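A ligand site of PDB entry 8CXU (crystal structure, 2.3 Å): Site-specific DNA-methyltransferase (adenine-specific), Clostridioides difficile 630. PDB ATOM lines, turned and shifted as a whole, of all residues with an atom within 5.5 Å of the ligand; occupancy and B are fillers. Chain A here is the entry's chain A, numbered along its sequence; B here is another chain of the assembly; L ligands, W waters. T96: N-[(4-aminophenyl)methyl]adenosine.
Residues that only touch the ligand: Ser 63, Tyr 179, Pro 168, DA 8 of chain B, Tyr 31, Cys 149, Ile 62, Phe 201, Gly 65, Asn 166 and Asp 117.
The backbone NH (N) of Leu 152 lies within hydrogen-bond range of the side-chain carboxylate (OD1) of Asp 150 (3.0 Å).
The backbone NH (N) of Cys 149 lies within hydrogen-bond range of the backbone carbonyl oxygen (O) of Asp 115, at 3.1 Å.
The side-chain carboxylate (OD2) of Asp 115 lies within hydrogen-bond range of the backbone NH (N) of Gly 65, 2.7 Å away.
The backbone NH of Asp 117 sits at hydrogen-bond distance from the side-chain carboxylate of Asp 115 (2.9 Å).
O of Ile 62 lies within hydrogen-bond range of OG of Ser 151.
OG of Ser 63 sits at hydrogen-bond distance from O of Asn 166.
The backbone NH (N) of Ile 116 sits close to the backbone carbonyl oxygen (O) of Cys 149 (3.4 Å).
The side-chain amide nitrogen (ND2) of Asn 166 is in hydrogen-bond range of N1 of DA 8 of chain B, at 3.0 Å.
OD1 of Asp 150 lies within hydrogen-bond range of N4 of the ligand (2.5 Å).
O3 of the ligand lies within hydrogen-bond range of OD1 of Asp 115, 2.5 Å away.
N of Ser 151 is in hydrogen-bond range of N3 of the ligand, 2.9 Å away.
The backbone carbonyl oxygen (O) of Gly 29 is in hydrogen-bond range of an oxygen (O2) of the ligand (3.3 Å).
A nitrogen (N2) of the ligand lies within hydrogen-bond range of the backbone NH of Ile 116 (3.3 Å).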
ATOM      1  N   GLY A  29      33.770   1.943 -24.433  1.00  0.00           N
ATOM      2  CA  GLY A  29      32.586   1.157 -24.124  1.00  0.00           C
ATOM      3  C   GLY A  29      31.315   1.664 -24.779  1.00  0.00           C
ATOM      4  O   GLY A  29      30.245   1.072 -24.595  1.00  0.00           O
ATOM      5  N   ILE A  30      31.418   2.744 -25.538  1.00  0.00           N
ATOM      6  CA  ILE A  30      30.288   3.359 -26.215  1.00  0.00           C
ATOM      7  C   ILE A  30      30.538   3.322 -27.717  1.00  0.00           C
ATOM      8  O   ILE A  30      31.588   3.766 -28.180  1.00  0.00           O
ATOM      9  CB  ILE A  30      30.048   4.801 -25.731  1.00  0.00           C
ATOM     10  N   TYR A  31      29.561   2.800 -28.462  1.00  0.00           N
ATOM     11  CA  TYR A  31      29.668   2.622 -29.907  1.00  0.00           C
ATOM     12  C   TYR A  31      28.608   3.466 -30.616  1.00  0.00           C
ATOM     13  O   TYR A  31      27.449   3.494 -30.197  1.00  0.00           O
ATOM     14  CB  TYR A  31      29.500   1.149 -30.289  1.00  0.00           C
ATOM     15  CG  TYR A  31      30.538   0.228 -29.678  1.00  0.00           C
ATOM     16  CD1 TYR A  31      30.350  -0.325 -28.424  1.00  0.00           C
ATOM     17  CD2 TYR A  31      31.711  -0.081 -30.369  1.00  0.00           C
ATOM     18  CE1 TYR A  31      31.292  -1.172 -27.863  1.00  0.00           C
ATOM     19  CE2 TYR A  31      32.656  -0.918 -29.822  1.00  0.00           C
ATOM     20  CZ  TYR A  31      32.443  -1.467 -28.569  1.00  0.00           C
ATOM     21  OH  TYR A  31      33.393  -2.296 -28.022  1.00  0.00           O
ATOM     22  N   ILE A  62      17.198   0.686 -23.916  1.00  0.00           N
ATOM     23  CA  ILE A  62      17.796   0.215 -22.666  1.00  0.00           C
ATOM     24  C   ILE A  62      19.316   0.221 -22.686  1.00  0.00           C
ATOM     25  O   ILE A  62      19.945  -0.167 -21.698  1.00  0.00           O
ATOM     26  CB  ILE A  62      17.320  -1.193 -22.282  1.00  0.00           C
ATOM     27  CG1 ILE A  62      17.556  -2.190 -23.414  1.00  0.00           C
ATOM     28  CG2 ILE A  62      15.857  -1.178 -21.894  1.00  0.00           C
ATOM     29  CD1 ILE A  62      17.090  -3.582 -23.066  1.00  0.00           C
ATOM     30  N   SER A  63      19.929   0.629 -23.793  1.00  0.00           N
ATOM     31  CA  SER A  63      21.362   0.886 -23.855  1.00  0.00           C
ATOM     32  C   SER A  63      21.592   2.195 -24.607  1.00  0.00           C
ATOM     33  O   SER A  63      22.381   2.275 -25.555  1.00  0.00           O
ATOM     34  CB  SER A  63      22.116  -0.286 -24.494  1.00  0.00           C
ATOM     35  OG  SER A  63      21.494  -0.703 -25.685  1.00  0.00           O
ATOM     36  N   CYS A  64      20.879   3.240 -24.181  1.00  0.00           N
ATOM     37  CA  CYS A  64      20.748   4.465 -24.965  1.00  0.00           C
ATOM     38  C   CYS A  64      22.069   5.176 -25.182  1.00  0.00           C
ATOM     39  O   CYS A  64      22.229   5.900 -26.164  1.00  0.00           O
ATOM     40  CB  CYS A  64      19.745   5.408 -24.296  1.00  0.00           C
ATOM     41  SG  CYS A  64      20.235   5.909 -22.626  1.00  0.00           S
ATOM     42  N   GLY A  65      23.031   4.992 -24.268  1.00  0.00           N
ATOM     43  CA  GLY A  65      24.286   5.704 -24.411  1.00  0.00           C
ATOM     44  C   GLY A  65      24.073   7.208 -24.359  1.00  0.00           C
ATOM     45  O   GLY A  65      23.378   7.737 -23.484  1.00  0.00           O
ATOM     46  N   ALA A 114      17.902   3.955 -20.646  1.00  0.00           N
ATOM     47  CA  ALA A 114      18.703   3.332 -19.605  1.00  0.00           C
ATOM     48  C   ALA A 114      20.103   3.060 -20.135  1.00  0.00           C
ATOM     49  O   ALA A 114      20.263   2.648 -21.280  1.00  0.00           O
ATOM     50  CB  ALA A 114      18.062   2.032 -19.105  1.00  0.00           C
ATOM     51  N   ASP A 115      21.104   3.294 -19.292  1.00  0.00           N
ATOM     52  CA  ASP A 115      22.471   2.947 -19.646  1.00  0.00           C
ATOM     53  C   ASP A 115      23.297   2.843 -18.371  1.00  0.00           C
ATOM     54  O   ASP A 115      23.022   3.530 -17.384  1.00  0.00           O
ATOM     55  CB  ASP A 115      23.080   3.973 -20.604  1.00  0.00           C
ATOM     56  CG  ASP A 115      24.250   3.405 -21.385  1.00  0.00           C
ATOM     57  OD1 ASP A 115      25.326   3.174 -20.774  1.00  0.00           O
ATOM     58  OD2 ASP A 115      24.087   3.171 -22.596  1.00  0.00           O
ATOM     59  N   ILE A 116      24.310   1.982 -18.413  1.00  0.00           N
ATOM     60  CA  ILE A 116      25.165   1.791 -17.256  1.00  0.00           C
ATOM     61  C   ILE A 116      26.154   2.946 -17.072  1.00  0.00           C
ATOM     62  O   ILE A 116      26.621   3.186 -15.955  1.00  0.00           O
ATOM     63  CB  ILE A 116      25.910   0.441 -17.376  1.00  0.00           C
ATOM     64  CG1 ILE A 116      26.555   0.052 -16.042  1.00  0.00           C
ATOM     65  CG2 ILE A 116      26.936   0.482 -18.501  1.00  0.00           C
ATOM     66  CD1 ILE A 116      25.572  -0.127 -14.926  1.00  0.00           C
ATOM     67  N   ASP A 117      26.447   3.695 -18.143  1.00  0.00           N
ATOM     68  CA  ASP A 117      27.456   4.755 -18.112  1.00  0.00           C
ATOM     69  C   ASP A 117      26.802   6.054 -17.639  1.00  0.00           C
ATOM     70  O   ASP A 117      25.954   6.622 -18.330  1.00  0.00           O
ATOM     71  CB  ASP A 117      28.089   4.926 -19.481  1.00  0.00           C
ATOM     72  CG  ASP A 117      29.114   6.055 -19.528  1.00  0.00           C
ATOM     73  OD1 ASP A 117      29.543   6.523 -18.445  1.00  0.00           O
ATOM     74  OD2 ASP A 117      29.487   6.468 -20.643  1.00  0.00           O
ATOM     75  N   CYS A 149      21.692   2.560 -14.729  1.00  0.00           N
ATOM     76  CA  CYS A 149      21.522   1.264 -14.070  1.00  0.00           C
ATOM     77  C   CYS A 149      21.953   0.170 -15.040  1.00  0.00           C
ATOM     78  O   CYS A 149      22.327   0.435 -16.191  1.00  0.00           O
ATOM     79  CB  CYS A 149      20.075   1.053 -13.635  1.00  0.00           C
ATOM     80  SG  CYS A 149      18.949   0.784 -15.035  1.00  0.00           S
ATOM     81  N   ASP A 150      21.893  -1.066 -14.562  1.00  0.00           N
ATOM     82  CA  ASP A 150      22.054  -2.247 -15.403  1.00  0.00           C
ATOM     83  C   ASP A 150      20.657  -2.671 -15.855  1.00  0.00           C
ATOM     84  O   ASP A 150      19.846  -3.132 -15.042  1.00  0.00           O
ATOM     85  CB  ASP A 150      22.766  -3.360 -14.638  1.00  0.00           C
ATOM     86  CG  ASP A 150      22.871  -4.657 -15.425  1.00  0.00           C
ATOM     87  OD1 ASP A 150      22.489  -4.692 -16.615  1.00  0.00           O
ATOM     88  OD2 ASP A 150      23.329  -5.657 -14.844  1.00  0.00           O
ATOM     89  N   SER A 151      20.387  -2.523 -17.156  1.00  0.00           N
ATOM     90  CA  SER A 151      19.058  -2.816 -17.685  1.00  0.00           C
ATOM     91  C   SER A 151      18.653  -4.270 -17.461  1.00  0.00           C
ATOM     92  O   SER A 151      17.459  -4.571 -17.446  1.00  0.00           O
ATOM     93  CB  SER A 151      18.995  -2.482 -19.171  1.00  0.00           C
ATOM     94  OG  SER A 151      19.282  -1.117 -19.406  1.00  0.00           O
ATOM     95  N   LEU A 152      19.621  -5.172 -17.298  1.00  0.00           N
ATOM     96  CA  LEU A 152      19.311  -6.582 -17.092  1.00  0.00           C
ATOM     97  C   LEU A 152      18.924  -6.892 -15.650  1.00  0.00           C
ATOM     98  O   LEU A 152      18.411  -7.980 -15.392  1.00  0.00           O
ATOM     99  CB  LEU A 152      20.503  -7.444 -17.505  1.00  0.00           C
ATOM    100  CG  LEU A 152      20.836  -7.367 -19.002  1.00  0.00           C
ATOM    101  CD1 LEU A 152      21.933  -8.354 -19.353  1.00  0.00           C
ATOM    102  CD2 LEU A 152      19.587  -7.614 -19.837  1.00  0.00           C
ATOM    103  N   ASN A 166      20.752  -0.161 -29.793  1.00  0.00           N
ATOM    104  CA  ASN A 166      21.917  -0.986 -30.116  1.00  0.00           C
ATOM    105  C   ASN A 166      22.493  -1.548 -28.819  1.00  0.00           C
ATOM    106  O   ASN A 166      23.211  -0.827 -28.095  1.00  0.00           O
ATOM    107  CB  ASN A 166      22.952  -0.177 -30.876  1.00  0.00           C
ATOM    108  CG  ASN A 166      24.194  -0.970 -31.199  1.00  0.00           C
ATOM    109  OD1 ASN A 166      24.190  -2.201 -31.188  1.00  0.00           O
ATOM    110  ND2 ASN A 166      25.282  -0.265 -31.522  1.00  0.00           N
ATOM    111  N   PRO A 167      22.209  -2.799 -28.486  1.00  0.00           N
ATOM    112  CA  PRO A 167      22.636  -3.357 -27.190  1.00  0.00           C
ATOM    113  C   PRO A 167      24.129  -3.620 -27.178  1.00  0.00           C
ATOM    114  O   PRO A 167      24.788  -3.615 -28.226  1.00  0.00           O
ATOM    115  CB  PRO A 167      21.840  -4.662 -27.098  1.00  0.00           C
ATOM    116  CG  PRO A 167      21.668  -5.073 -28.514  1.00  0.00           C
ATOM    117  CD  PRO A 167      21.476  -3.794 -29.300  1.00  0.00           C
ATOM    118  N   PRO A 168      24.715  -3.821 -26.002  1.00  0.00           N
ATOM    119  CA  PRO A 168      26.122  -4.229 -25.940  1.00  0.00           C
ATOM    120  C   PRO A 168      26.317  -5.663 -26.412  1.00  0.00           C
ATOM    121  O   PRO A 168      25.498  -6.541 -26.119  1.00  0.00           O
ATOM    122  CB  PRO A 168      26.476  -4.083 -24.455  1.00  0.00           C
ATOM    123  CG  PRO A 168      25.175  -4.243 -23.750  1.00  0.00           C
ATOM    124  CD  PRO A 168      24.145  -3.613 -24.654  1.00  0.00           C
ATOM    125  N   ILE A 170      28.964  -8.603 -25.872  1.00  0.00           N
ATOM    126  CA  ILE A 170      30.102  -9.085 -25.103  1.00  0.00           C
ATOM    127  C   ILE A 170      30.081 -10.609 -25.116  1.00  0.00           C
ATOM    128  O   ILE A 170      29.115 -11.218 -24.645  1.00  0.00           O
ATOM    129  CB  ILE A 170      30.112  -8.562 -23.652  1.00  0.00           C
ATOM    130  CG1 ILE A 170      30.075  -7.034 -23.632  1.00  0.00           C
ATOM    131  CG2 ILE A 170      31.347  -9.064 -22.923  1.00  0.00           C
ATOM    132  CD1 ILE A 170      30.053  -6.432 -22.239  1.00  0.00           C
ATOM    133  N   LEU A 175      33.475 -11.372 -20.883  1.00  0.00           N
ATOM    134  CA  LEU A 175      32.462 -11.149 -19.852  1.00  0.00           C
ATOM    135  C   LEU A 175      32.969 -11.662 -18.511  1.00  0.00           C
ATOM    136  O   LEU A 175      33.603 -12.718 -18.445  1.00  0.00           O
ATOM    137  CB  LEU A 175      31.155 -11.847 -20.228  1.00  0.00           C
ATOM    138  CG  LEU A 175      29.852 -11.368 -19.592  1.00  0.00           C
ATOM    139  CD1 LEU A 175      29.735  -9.853 -19.686  1.00  0.00           C
ATOM    140  CD2 LEU A 175      28.668 -12.036 -20.273  1.00  0.00           C
ATOM    141  N   TYR A 179      29.555 -11.959 -13.313  1.00  0.00           N
ATOM    142  CA  TYR A 179      28.349 -11.548 -14.029  1.00  0.00           C
ATOM    143  C   TYR A 179      27.725 -12.710 -14.775  1.00  0.00           C
ATOM    144  O   TYR A 179      26.491 -12.832 -14.835  1.00  0.00           O
ATOM    145  CB  TYR A 179      28.669 -10.400 -14.993  1.00  0.00           C
ATOM    146  CG  TYR A 179      27.453  -9.612 -15.414  1.00  0.00           C
ATOM    147  CD1 TYR A 179      26.955  -8.592 -14.611  1.00  0.00           C
ATOM    148  CD2 TYR A 179      26.782  -9.898 -16.596  1.00  0.00           C
ATOM    149  CE1 TYR A 179      25.848  -7.875 -14.977  1.00  0.00           C
ATOM    150  CE2 TYR A 179      25.667  -9.189 -16.976  1.00  0.00           C
ATOM    151  CZ  TYR A 179      25.200  -8.177 -16.166  1.00  0.00           C
ATOM    152  OH  TYR A 179      24.089  -7.457 -16.524  1.00  0.00           O
ATOM    153  N   LEU A 197      26.184 -11.621 -24.429  1.00  0.00           N
ATOM    154  CA  LEU A 197      25.396 -10.728 -23.584  1.00  0.00           C
ATOM    155  C   LEU A 197      24.176 -10.188 -24.320  1.00  0.00           C
ATOM    156  O   LEU A 197      23.111  -9.994 -23.710  1.00  0.00           O
ATOM    157  CB  LEU A 197      26.270  -9.582 -23.089  1.00  0.00           C
ATOM    158  CG  LEU A 197      25.615  -8.511 -22.214  1.00  0.00           C
ATOM    159  CD1 LEU A 197      25.201  -9.075 -20.863  1.00  0.00           C
ATOM    160  CD2 LEU A 197      26.558  -7.336 -22.025  1.00  0.00           C
ATOM    161  N   PHE A 201      19.682  -9.142 -23.749  1.00  0.00           N
ATOM    162  CA  PHE A 201      18.960  -7.923 -24.092  1.00  0.00           C
ATOM    163  C   PHE A 201      17.781  -8.223 -25.016  1.00  0.00           C
ATOM    164  O   PHE A 201      16.716  -7.612 -24.891  1.00  0.00           O
ATOM    165  CB  PHE A 201      19.907  -6.900 -24.730  1.00  0.00           C
ATOM    166  CG  PHE A 201      20.684  -6.104 -23.727  1.00  0.00           C
ATOM    167  CD1 PHE A 201      21.764  -6.674 -23.056  1.00  0.00           C
ATOM    168  CD2 PHE A 201      20.339  -4.798 -23.451  1.00  0.00           C
ATOM    169  CE1 PHE A 201      22.472  -5.933 -22.123  1.00  0.00           C
ATOM    170  CE2 PHE A 201      21.047  -4.057 -22.518  1.00  0.00           C
ATOM    171  CZ  PHE A 201      22.124  -4.625 -21.860  1.00  0.00           C
ATOM    172  P    DA B   8      33.880 -10.499 -30.286  1.00  0.00           P
ATOM    173  OP1  DA B   8      35.192 -10.107 -29.722  1.00  0.00           O
ATOM    174  OP2  DA B   8      32.808 -10.983 -29.376  1.00  0.00           O
ATOM    175  O5'  DA B   8      33.302  -9.291 -31.154  1.00  0.00           O
ATOM    176  C5'  DA B   8      32.585  -8.243 -30.544  1.00  0.00           C
ATOM    177  C4'  DA B   8      32.804  -6.964 -31.326  1.00  0.00           C
ATOM    178  O4'  DA B   8      31.605  -6.147 -31.295  1.00  0.00           O
ATOM    179  C3'  DA B   8      33.932  -6.088 -30.809  1.00  0.00           C
ATOM    180  O3'  DA B   8      34.634  -5.521 -31.900  1.00  0.00           O
ATOM    181  C2'  DA B   8      33.182  -5.017 -30.013  1.00  0.00           C
ATOM    182  C1'  DA B   8      31.944  -4.848 -30.862  1.00  0.00           C
ATOM    183  N9   DA B   8      30.799  -4.303 -30.155  1.00  0.00           N
ATOM    184  C8   DA B   8      30.428  -4.536 -28.862  1.00  0.00           C
ATOM    185  N7   DA B   8      29.337  -3.916 -28.496  1.00  0.00           N
ATOM    186  C5   DA B   8      28.957  -3.210 -29.629  1.00  0.00           C
ATOM    187  C6   DA B   8      27.876  -2.347 -29.900  1.00  0.00           C
ATOM    188  N6   DA B   8      26.943  -2.030 -28.995  1.00  0.00           N
ATOM    189  N1   DA B   8      27.802  -1.820 -31.138  1.00  0.00           N
ATOM    190  C2   DA B   8      28.740  -2.129 -32.042  1.00  0.00           C
ATOM    191  N3   DA B   8      29.789  -2.930 -31.904  1.00  0.00           N
ATOM    192  C4   DA B   8      29.850  -3.436 -30.668  1.00  0.00           C
HETATM  193  C1  T96 L   1      25.785   0.574 -24.680  1.00  0.00           C
HETATM  194  C2  T96 L   1      25.606   0.128 -22.425  1.00  0.00           C
HETATM  195  C3  T96 L   1      26.405  -2.043 -21.368  1.00  0.00           C
HETATM  196  N4  T96 L   1      23.995  -4.203 -18.505  1.00  0.00           N
HETATM  197  C5  T96 L   1      24.505  -1.272 -20.619  1.00  0.00           C
HETATM  198  C6  T96 L   1      22.649  -1.084 -19.441  1.00  0.00           C
HETATM  199  C7  T96 L   1      23.894  -2.985 -19.085  1.00  0.00           C
HETATM  200  C8  T96 L   1      25.053  -5.159 -18.793  1.00  0.00           C
HETATM  201  C11 T96 L   1      28.382  -5.861 -17.109  1.00  0.00           C
HETATM  202  C10 T96 L   1      27.304  -5.923 -17.982  1.00  0.00           C
HETATM  203  C9  T96 L   1      26.215  -5.088 -17.837  1.00  0.00           C
HETATM  204  C12 T96 L   1      28.384  -4.946 -16.056  1.00  0.00           C
HETATM  205  C15 T96 L   1      26.207  -0.191 -25.908  1.00  0.00           C
HETATM  206  C16 T96 L   1      26.991   0.726 -22.580  1.00  0.00           C
HETATM  207  N   T96 L   1      25.532  -0.997 -21.495  1.00  0.00           N
HETATM  208  C   T96 L   1      26.894   1.367 -23.977  1.00  0.00           C
HETATM  209  O   T96 L   1      26.569   2.755 -23.909  1.00  0.00           O
HETATM  210  C13 T96 L   1      27.274  -4.109 -15.899  1.00  0.00           C
HETATM  211  C14 T96 L   1      26.212  -4.183 -16.784  1.00  0.00           C
HETATM  212  C4  T96 L   1      24.827  -2.482 -20.033  1.00  0.00           C
HETATM  213  N1  T96 L   1      26.036  -2.960 -20.515  1.00  0.00           N
HETATM  214  N2  T96 L   1      23.426  -0.522 -20.367  1.00  0.00           N
HETATM  215  N3  T96 L   1      22.811  -2.243 -18.797  1.00  0.00           N
HETATM  216  N5  T96 L   1      29.444  -4.872 -15.185  1.00  0.00           N
HETATM  217  O1  T96 L   1      25.244  -0.338 -23.698  1.00  0.00           O
HETATM  218  O2  T96 L   1      27.579   0.031 -26.207  1.00  0.00           O
HETATM  219  O3  T96 L   1      27.218   1.702 -21.575  1.00  0.00           O
HETATM  220  O   HOH W   1      29.379  -3.445 -19.653  1.00  0.00           O
